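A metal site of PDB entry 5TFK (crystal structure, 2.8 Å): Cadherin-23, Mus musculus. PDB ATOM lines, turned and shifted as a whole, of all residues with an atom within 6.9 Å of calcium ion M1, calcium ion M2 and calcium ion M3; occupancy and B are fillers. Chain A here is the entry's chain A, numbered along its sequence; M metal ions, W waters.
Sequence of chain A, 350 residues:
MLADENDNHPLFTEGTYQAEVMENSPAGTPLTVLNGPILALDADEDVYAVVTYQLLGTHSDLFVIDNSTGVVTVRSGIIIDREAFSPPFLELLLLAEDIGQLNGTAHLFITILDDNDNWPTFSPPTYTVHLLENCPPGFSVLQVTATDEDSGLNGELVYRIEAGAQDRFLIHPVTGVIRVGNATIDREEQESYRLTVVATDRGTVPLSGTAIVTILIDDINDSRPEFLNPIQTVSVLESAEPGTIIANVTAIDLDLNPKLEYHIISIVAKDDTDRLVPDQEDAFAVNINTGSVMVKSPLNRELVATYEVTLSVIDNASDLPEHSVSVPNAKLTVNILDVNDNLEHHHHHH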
ATOM      1  N   GLU A 133       9.805   1.111 -27.066  1.00  0.00           N
ATOM      2  CA  GLU A 133      10.955   1.878 -26.549  1.00  0.00           C
ATOM      3  C   GLU A 133      11.115   1.893 -25.013  1.00  0.00           C
ATOM      4  O   GLU A 133      10.206   1.501 -24.248  1.00  0.00           O
ATOM      5  CB  GLU A 133      10.966   3.329 -27.092  1.00  0.00           C
ATOM      6  CG  GLU A 133       9.894   4.278 -26.537  1.00  0.00           C
ATOM      7  CD  GLU A 133      10.078   5.742 -26.931  1.00  0.00           C
ATOM      8  OE1 GLU A 133      11.161   6.313 -26.708  1.00  0.00           O
ATOM      9  OE2 GLU A 133       9.116   6.363 -27.406  1.00  0.00           O
ATOM     10  N   ASN A 134      12.300   2.367 -24.589  1.00  0.00           N
ATOM     11  CA  ASN A 134      12.738   2.383 -23.178  1.00  0.00           C
ATOM     12  C   ASN A 134      12.734   0.988 -22.560  1.00  0.00           C
ATOM     13  O   ASN A 134      12.219   0.750 -21.474  1.00  0.00           O
ATOM     14  CB  ASN A 134      11.848   3.306 -22.337  1.00  0.00           C
ATOM     15  CG  ASN A 134      11.798   4.700 -22.876  1.00  0.00           C
ATOM     16  OD1 ASN A 134      12.839   5.296 -23.130  1.00  0.00           O
ATOM     17  ND2 ASN A 134      10.590   5.221 -23.054  1.00  0.00           N
ATOM     18  N   ILE A 185      17.001   2.388 -25.944  1.00  0.00           N
ATOM     19  CA  ILE A 185      16.268   2.452 -27.203  1.00  0.00           C
ATOM     20  C   ILE A 185      15.269   3.570 -27.149  1.00  0.00           C
ATOM     21  O   ILE A 185      14.194   3.410 -26.571  1.00  0.00           O
ATOM     22  CB  ILE A 185      15.512   1.139 -27.479  1.00  0.00           C
ATOM     23  CG1 ILE A 185      16.506  -0.019 -27.647  1.00  0.00           C
ATOM     24  CG2 ILE A 185      14.585   1.242 -28.691  1.00  0.00           C
ATOM     25  CD1 ILE A 185      17.687   0.281 -28.555  1.00  0.00           C
ATOM     26  N   ASP A 186      15.630   4.712 -27.733  1.00  0.00           N
ATOM     27  CA  ASP A 186      14.754   5.882 -27.772  1.00  0.00           C
ATOM     28  C   ASP A 186      14.211   6.013 -29.170  1.00  0.00           C
ATOM     29  O   ASP A 186      14.982   6.252 -30.089  1.00  0.00           O
ATOM     30  CB  ASP A 186      15.572   7.132 -27.434  1.00  0.00           C
ATOM     31  CG  ASP A 186      14.720   8.383 -27.317  1.00  0.00           C
ATOM     32  OD1 ASP A 186      13.488   8.304 -27.422  1.00  0.00           O
ATOM     33  OD2 ASP A 186      15.316   9.465 -27.104  1.00  0.00           O
ATOM     34  N   ARG A 187      12.897   5.870 -29.315  1.00  0.00           N
ATOM     35  CA  ARG A 187      12.233   6.076 -30.606  1.00  0.00           C
ATOM     36  C   ARG A 187      12.490   7.437 -31.224  1.00  0.00           C
ATOM     37  O   ARG A 187      12.512   7.566 -32.446  1.00  0.00           O
ATOM     38  CB  ARG A 187      10.721   5.930 -30.474  1.00  0.00           C
ATOM     39  CG  ARG A 187      10.037   5.556 -31.785  1.00  0.00           C
ATOM     40  CD  ARG A 187       8.560   5.857 -31.742  1.00  0.00           C
ATOM     41  NE  ARG A 187       8.394   7.305 -31.722  1.00  0.00           N
ATOM     42  CZ  ARG A 187       8.297   8.076 -32.794  1.00  0.00           C
ATOM     43  NH1 ARG A 187       8.263   7.559 -34.025  1.00  0.00           N
ATOM     44  NH2 ARG A 187       8.177   9.388 -32.617  1.00  0.00           N
ATOM     45  N   GLU A 188      12.650   8.452 -30.389  1.00  0.00           N
ATOM     46  CA  GLU A 188      12.963   9.799 -30.867  1.00  0.00           C
ATOM     47  C   GLU A 188      14.411   9.918 -31.388  1.00  0.00           C
ATOM     48  O   GLU A 188      14.702  10.810 -32.184  1.00  0.00           O
ATOM     49  CB  GLU A 188      12.690  10.821 -29.765  1.00  0.00           C
ATOM     50  CG  GLU A 188      11.224  11.210 -29.594  1.00  0.00           C
ATOM     51  CD  GLU A 188      10.323  10.081 -29.128  1.00  0.00           C
ATOM     52  OE1 GLU A 188       9.530   9.530 -29.932  1.00  0.00           O
ATOM     53  OE2 GLU A 188      10.371   9.741 -27.928  1.00  0.00           O
ATOM     54  N   GLU A 189      15.299   9.032 -30.940  1.00  0.00           N
ATOM     55  CA  GLU A 189      16.659   8.946 -31.499  1.00  0.00           C
ATOM     56  C   GLU A 189      16.665   8.220 -32.842  1.00  0.00           C
ATOM     57  O   GLU A 189      17.341   8.625 -33.784  1.00  0.00           O
ATOM     58  CB  GLU A 189      17.628   8.245 -30.522  1.00  0.00           C
ATOM     59  CG  GLU A 189      19.042   8.062 -31.066  1.00  0.00           C
ATOM     60  CD  GLU A 189      20.055   7.721 -30.000  1.00  0.00           C
ATOM     61  OE1 GLU A 189      21.165   8.281 -30.048  1.00  0.00           O
ATOM     62  OE2 GLU A 189      19.752   6.874 -29.129  1.00  0.00           O
ATOM     63  N   ASP A 218       8.041   1.252 -31.121  1.00  0.00           N
ATOM     64  CA  ASP A 218       6.722   1.747 -30.860  1.00  0.00           C
ATOM     65  C   ASP A 218       6.939   2.849 -29.867  1.00  0.00           C
ATOM     66  O   ASP A 218       7.946   2.874 -29.154  1.00  0.00           O
ATOM     67  CB  ASP A 218       5.819   0.645 -30.321  1.00  0.00           C
ATOM     68  CG  ASP A 218       5.351  -0.278 -31.406  1.00  0.00           C
ATOM     69  OD1 ASP A 218       5.723  -0.044 -32.572  1.00  0.00           O
ATOM     70  OD2 ASP A 218       4.614  -1.236 -31.127  1.00  0.00           O
ATOM     71  N   ASP A 219       6.014   3.793 -29.834  1.00  0.00           N
ATOM     72  CA  ASP A 219       6.181   5.034 -29.064  1.00  0.00           C
ATOM     73  C   ASP A 219       5.571   4.926 -27.666  1.00  0.00           C
ATOM     74  O   ASP A 219       4.462   4.425 -27.490  1.00  0.00           O
ATOM     75  CB  ASP A 219       5.560   6.181 -29.833  1.00  0.00           C
ATOM     76  CG  ASP A 219       5.805   7.508 -29.196  1.00  0.00           C
ATOM     77  OD1 ASP A 219       6.971   7.941 -29.115  1.00  0.00           O
ATOM     78  OD2 ASP A 219       4.808   8.120 -28.765  1.00  0.00           O
ATOM     79  N   ILE A 220       6.367   5.328 -26.682  1.00  0.00           N
ATOM     80  CA  ILE A 220       5.821   5.826 -25.439  1.00  0.00           C
ATOM     81  C   ILE A 220       5.943   7.350 -25.562  1.00  0.00           C
ATOM     82  O   ILE A 220       6.930   7.858 -26.096  1.00  0.00           O
ATOM     83  CB  ILE A 220       6.609   5.316 -24.210  1.00  0.00           C
ATOM     84  CG1 ILE A 220       6.625   3.780 -24.147  1.00  0.00           C
ATOM     85  CG2 ILE A 220       5.987   5.862 -22.938  1.00  0.00           C
ATOM     86  CD1 ILE A 220       7.649   3.212 -23.165  1.00  0.00           C
ATOM     87  N   ASN A 221       4.913   8.067 -25.101  1.00  0.00           N
ATOM     88  CA  ASN A 221       4.965   9.527 -25.037  1.00  0.00           C
ATOM     89  C   ASN A 221       5.844   9.960 -23.866  1.00  0.00           C
ATOM     90  O   ASN A 221       5.364  10.231 -22.763  1.00  0.00           O
ATOM     91  CB  ASN A 221       3.563  10.114 -24.916  1.00  0.00           C
ATOM     92  CG  ASN A 221       3.548  11.605 -25.124  1.00  0.00           C
ATOM     93  OD1 ASN A 221       4.336  12.328 -24.517  1.00  0.00           O
ATOM     94  ND2 ASN A 221       2.676  12.076 -25.997  1.00  0.00           N
ATOM     95  N   ASP A 222       7.143   9.999 -24.102  1.00  0.00           N
ATOM     96  CA  ASP A 222       8.116  10.115 -23.042  1.00  0.00           C
ATOM     97  C   ASP A 222       9.002  11.317 -23.225  1.00  0.00           C
ATOM     98  O   ASP A 222       9.995  11.461 -22.528  1.00  0.00           O
ATOM     99  CB  ASP A 222       8.974   8.831 -22.977  1.00  0.00           C
ATOM    100  CG  ASP A 222       9.824   8.624 -24.228  1.00  0.00           C
ATOM    101  OD1 ASP A 222       9.549   9.218 -25.287  1.00  0.00           O
ATOM    102  OD2 ASP A 222      10.763   7.828 -24.146  1.00  0.00           O
ATOM    103  N   SER A 223       8.620  12.196 -24.144  1.00  0.00           N
ATOM    104  CA  SER A 223       9.498  13.264 -24.581  1.00  0.00           C
ATOM    105  C   SER A 223       8.815  14.594 -24.297  1.00  0.00           C
ATOM    106  O   SER A 223       7.689  14.815 -24.741  1.00  0.00           O
ATOM    107  CB  SER A 223       9.784  13.123 -26.067  1.00  0.00           C
ATOM    108  OG  SER A 223      10.992  13.747 -26.403  1.00  0.00           O
ATOM    109  N   ARG A 224       9.481  15.443 -23.512  1.00  0.00           N
ATOM    110  CA  ARG A 224       8.893  16.697 -23.057  1.00  0.00           C
ATOM    111  C   ARG A 224       8.835  17.753 -24.165  1.00  0.00           C
ATOM    112  O   ARG A 224       9.775  17.901 -24.944  1.00  0.00           O
ATOM    113  CB  ARG A 224       9.630  17.253 -21.828  1.00  0.00           C
ATOM    114  CG  ARG A 224      10.923  18.012 -22.125  1.00  0.00           C
ATOM    115  CD  ARG A 224      11.460  18.746 -20.901  1.00  0.00           C
ATOM    116  NE  ARG A 224      12.115  17.874 -19.918  1.00  0.00           N
ATOM    117  CZ  ARG A 224      11.543  17.377 -18.829  1.00  0.00           C
ATOM    118  NH1 ARG A 224      10.266  17.609 -18.539  1.00  0.00           N
ATOM    119  NH2 ARG A 224      12.259  16.609 -18.014  1.00  0.00           N
ATOM    120  N   PRO A 225       7.748  18.523 -24.201  1.00  0.00           N
ATOM    121  CA  PRO A 225       7.712  19.637 -25.150  1.00  0.00           C
ATOM    122  C   PRO A 225       8.814  20.661 -24.900  1.00  0.00           C
ATOM    123  O   PRO A 225       9.214  20.961 -23.755  1.00  0.00           O
ATOM    124  CB  PRO A 225       6.304  20.226 -24.952  1.00  0.00           C
ATOM    125  CG  PRO A 225       5.850  19.775 -23.615  1.00  0.00           C
ATOM    126  CD  PRO A 225       6.540  18.476 -23.364  1.00  0.00           C
ATOM    127  N   ASP A 253       6.995  18.854 -29.829  1.00  0.00           N
ATOM    128  CA  ASP A 253       7.027  17.562 -29.122  1.00  0.00           C
ATOM    129  C   ASP A 253       7.224  16.412 -30.124  1.00  0.00           C
ATOM    130  O   ASP A 253       6.500  16.309 -31.083  1.00  0.00           O
ATOM    131  CB  ASP A 253       5.710  17.348 -28.366  1.00  0.00           C
ATOM    132  CG  ASP A 253       5.831  16.377 -27.176  1.00  0.00           C
ATOM    133  OD1 ASP A 253       5.896  15.148 -27.350  1.00  0.00           O
ATOM    134  OD2 ASP A 253       5.759  16.854 -26.031  1.00  0.00           O
ATOM    135  N   LEU A 254       8.247  15.604 -29.889  1.00  0.00           N
ATOM    136  CA  LEU A 254       8.713  14.643 -30.875  1.00  0.00           C
ATOM    137  C   LEU A 254       8.042  13.278 -30.754  1.00  0.00           C
ATOM    138  O   LEU A 254       8.339  12.381 -31.532  1.00  0.00           O
ATOM    139  CB  LEU A 254      10.226  14.476 -30.764  1.00  0.00           C
ATOM    140  CG  LEU A 254      11.023  15.767 -30.957  1.00  0.00           C
ATOM    141  CD1 LEU A 254      12.430  15.631 -30.377  1.00  0.00           C
ATOM    142  CD2 LEU A 254      11.052  16.146 -32.427  1.00  0.00           C
ATOM    143  N   ASP A 255       7.127  13.119 -29.802  1.00  0.00           N
ATOM    144  CA  ASP A 255       6.346  11.899 -29.683  1.00  0.00           C
ATOM    145  C   ASP A 255       5.251  11.876 -30.741  1.00  0.00           C
ATOM    146  O   ASP A 255       5.059  12.853 -31.457  1.00  0.00           O
ATOM    147  CB  ASP A 255       5.737  11.780 -28.276  1.00  0.00           C
ATOM    148  CG  ASP A 255       6.787  11.606 -27.203  1.00  0.00           C
ATOM    149  OD1 ASP A 255       7.625  10.679 -27.320  1.00  0.00           O
ATOM    150  OD2 ASP A 255       6.757  12.393 -26.219  1.00  0.00           O
ATOM    151  N   LEU A 256       4.511  10.772 -30.806  1.00  0.00           N
ATOM    152  CA  LEU A 256       3.675  10.497 -31.948  1.00  0.00           C
ATOM    153  C   LEU A 256       2.370  11.274 -31.978  1.00  0.00           C
ATOM    154  O   LEU A 256       1.947  11.663 -33.055  1.00  0.00           O
ATOM    155  CB  LEU A 256       3.425   8.994 -32.114  1.00  0.00           C
ATOM    156  CG  LEU A 256       4.396   8.284 -33.073  1.00  0.00           C
ATOM    157  CD1 LEU A 256       4.234   6.778 -33.028  1.00  0.00           C
ATOM    158  CD2 LEU A 256       4.231   8.749 -34.516  1.00  0.00           C
ATOM    159  N   PRO A 258       1.007  14.262 -29.735  1.00  0.00           N
ATOM    160  CA  PRO A 258       0.918  15.225 -28.645  1.00  0.00           C
ATOM    161  C   PRO A 258      -0.386  15.992 -28.690  1.00  0.00           C
ATOM    162  O   PRO A 258      -0.971  16.155 -29.762  1.00  0.00           O
ATOM    163  CB  PRO A 258       2.101  16.160 -28.901  1.00  0.00           C
ATOM    164  CG  PRO A 258       2.513  15.921 -30.299  1.00  0.00           C
ATOM    165  CD  PRO A 258       2.169  14.503 -30.600  1.00  0.00           C
ATOM    166  N   LEU A 260      -0.683  19.664 -27.221  1.00  0.00           N
ATOM    167  CA  LEU A 260       0.044  20.714 -26.554  1.00  0.00           C
ATOM    168  C   LEU A 260      -0.924  21.807 -26.094  1.00  0.00           C
ATOM    169  O   LEU A 260      -1.757  22.293 -26.870  1.00  0.00           O
ATOM    170  CB  LEU A 260       1.113  21.296 -27.468  1.00  0.00           C
ATOM    171  CG  LEU A 260       2.251  20.350 -27.896  1.00  0.00           C
ATOM    172  CD1 LEU A 260       3.389  21.101 -28.590  1.00  0.00           C
ATOM    173  CD2 LEU A 260       2.806  19.592 -26.719  1.00  0.00           C
ATOM    174  N   ASP A 315       2.269  18.600 -22.645  1.00  0.00           N
ATOM    175  CA  ASP A 315       1.688  17.527 -23.472  1.00  0.00           C
ATOM    176  C   ASP A 315       0.650  16.754 -22.668  1.00  0.00           C
ATOM    177  O   ASP A 315       1.016  16.169 -21.670  1.00  0.00           O
ATOM    178  CB  ASP A 315       2.825  16.593 -23.909  1.00  0.00           C
ATOM    179  CG  ASP A 315       2.439  15.685 -25.068  1.00  0.00           C
ATOM    180  OD1 ASP A 315       1.234  15.615 -25.394  1.00  0.00           O
ATOM    181  OD2 ASP A 315       3.348  15.026 -25.659  1.00  0.00           O
ATOM    182  N   ALA A 317      -1.028  14.241 -23.642  1.00  0.00           N
ATOM    183  CA  ALA A 317      -0.979  12.848 -24.003  1.00  0.00           C
ATOM    184  C   ALA A 317       0.204  12.183 -23.320  1.00  0.00           C
ATOM    185  O   ALA A 317       0.455  11.003 -23.564  1.00  0.00           O
ATOM    186  CB  ALA A 317      -0.874  12.712 -25.503  1.00  0.00           C
ATOM    187  N   SER A 318       0.913  12.890 -22.459  1.00  0.00           N
ATOM    188  CA  SER A 318       2.159  12.349 -21.916  1.00  0.00           C
ATOM    189  C   SER A 318       1.897  11.116 -21.063  1.00  0.00           C
ATOM    190  O   SER A 318       0.884  11.025 -20.363  1.00  0.00           O
ATOM    191  CB  SER A 318       2.934  13.418 -21.147  1.00  0.00           C
ATOM    192  OG  SER A 318       4.339  13.184 -21.232  1.00  0.00           O
ATOM    193  N   ASP A 319       2.788  10.139 -21.208  1.00  0.00           N
ATOM    194  CA  ASP A 319       2.638   8.844 -20.552  1.00  0.00           C
ATOM    195  C   ASP A 319       3.460   8.805 -19.273  1.00  0.00           C
ATOM    196  O   ASP A 319       3.168   8.030 -18.377  1.00  0.00           O
ATOM    197  CB  ASP A 319       3.053   7.705 -21.486  1.00  0.00           C
ATOM    198  CG  ASP A 319       2.002   7.387 -22.558  1.00  0.00           C
ATOM    199  OD1 ASP A 319       0.832   7.067 -22.208  1.00  0.00           O
ATOM    200  OD2 ASP A 319       2.343   7.424 -23.759  1.00  0.00           O
ATOM    201  N   HIS A 323       8.063  13.947 -17.904  1.00  0.00           N
ATOM    202  CA  HIS A 323       8.489  14.462 -19.224  1.00  0.00           C
ATOM    203  C   HIS A 323       7.306  15.087 -19.985  1.00  0.00           C
ATOM    204  O   HIS A 323       7.106  14.854 -21.198  1.00  0.00           O
ATOM    205  CB  HIS A 323       9.099  13.341 -20.076  1.00  0.00           C
ATOM    206  CG  HIS A 323      10.428  12.851 -19.597  1.00  0.00           C
ATOM    207  ND1 HIS A 323      11.009  11.685 -20.051  1.00  0.00           N
ATOM    208  CD2 HIS A 323      11.297  13.368 -18.695  1.00  0.00           C
ATOM    209  CE1 HIS A 323      12.171  11.506 -19.459  1.00  0.00           C
ATOM    210  NE2 HIS A 323      12.376  12.512 -18.631  1.00  0.00           N
ATOM    211  N   SER A 324       6.512  15.866 -19.258  1.00  0.00           N
ATOM    212  CA  SER A 324       5.248  16.338 -19.795  1.00  0.00           C
ATOM    213  C   SER A 324       5.098  17.841 -19.786  1.00  0.00           C
ATOM    214  O   SER A 324       4.182  18.327 -20.405  1.00  0.00           O
ATOM    215  CB  SER A 324       4.082  15.726 -19.017  1.00  0.00           C
ATOM    216  OG  SER A 324       3.990  16.309 -17.749  1.00  0.00           O
HETATM  217 CA    CA M   1       8.506   8.585 -27.537  1.00  0.00          CA
HETATM  218 CA    CA M   2      11.686   8.731 -26.270  1.00  0.00          CA
HETATM  219 CA    CA M   3       5.611  14.451 -25.038  1.00  0.00          CA
HETATM  220  O   HOH W   1      12.687   7.081 -25.321  1.00  0.00           O
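The side-chain carboxylate of Asp 219 sits close to the guanidinium group of Arg 187 (3.0 Å). OD2 of Asp 219 sits at hydrogen-bond distance from N of Leu 256 (3.4 Å). The backbone NH (N) of Arg 187 sits close to the side-chain carboxylate (OE1) of Glu 133. A ring nitrogen (ND1) of His 323 sits at hydrogen-bond distance from the backbone carbonyl oxygen of Asp 222, at 2.7 Å. ND2 of Asn 134 lies close to OD2 of Asp 222 (2.8 Å). N of Asp 315 is in hydrogen-bond range of O of Ser 324, 3.0 Å away. OG of Ser 318 is in hydrogen-bond range of O of Asn 221 (3.5 Å). The backbone NH of Asn 221 lies within hydrogen-bond range of the side-chain carboxylate of Asp 319 (3.0 Å).
OE2 of Glu 188 is bound to calcium ion M1 (2.2 Å). Calcium ion M1 is bound by O of Ile 220. OD1 of Asp 255 binds calcium ion M1, at 2.3 Å. OD1 of Asp 219 binds calcium ion M1 (2.3 Å). OE2 of Glu 133 is bound to calcium ion M1 (2.3 Å). Calcium ion M1 is bound by OD1 of Asp 222 (2.6 Å). The side-chain carboxylate (OE1) of Glu 188 binds calcium ion M1 (2.8 Å). Calcium ion M1 has seven donor atoms within binding distance.
Calcium ion M2 is bound by water W1 (2.2 Å), the side-chain carboxylate (OD1) of Asp 186 (2.2 Å), the side-chain carboxylate (OE2) of Glu 188 (2.3 Å), the side-chain carboxylate (OD1) of Asp 222 (2.4 Å), the side-chain carboxylate (OD2) of Asp 222 (2.5 Å) and the side-chain carboxylate (OE1) of Glu 133 (2.5 Å).
Calcium ion M3 is bound by the backbone carbonyl oxygen (O) of Ser 223 (2.1 Å), the side-chain carboxylate (OD2) of Asp 315 (2.4 Å), the side-chain carboxylate (OD1) of Asp 253 (2.4 Å), the side-chain amide oxygen (OD1) of Asn 221 (2.5 Å), the side-chain carboxylate (OD2) of Asp 253 (2.6 Å) and the side-chain carboxylate (OD2) of Asp 255 (2.6 Å). Calcium ion M3 has six donor atoms within binding distance.
Of the 27 residues printed, 4 come within 4 Å of calcium ion M2.
Of the 27 residues printed, 5 come within 4 Å of calcium ion M3.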
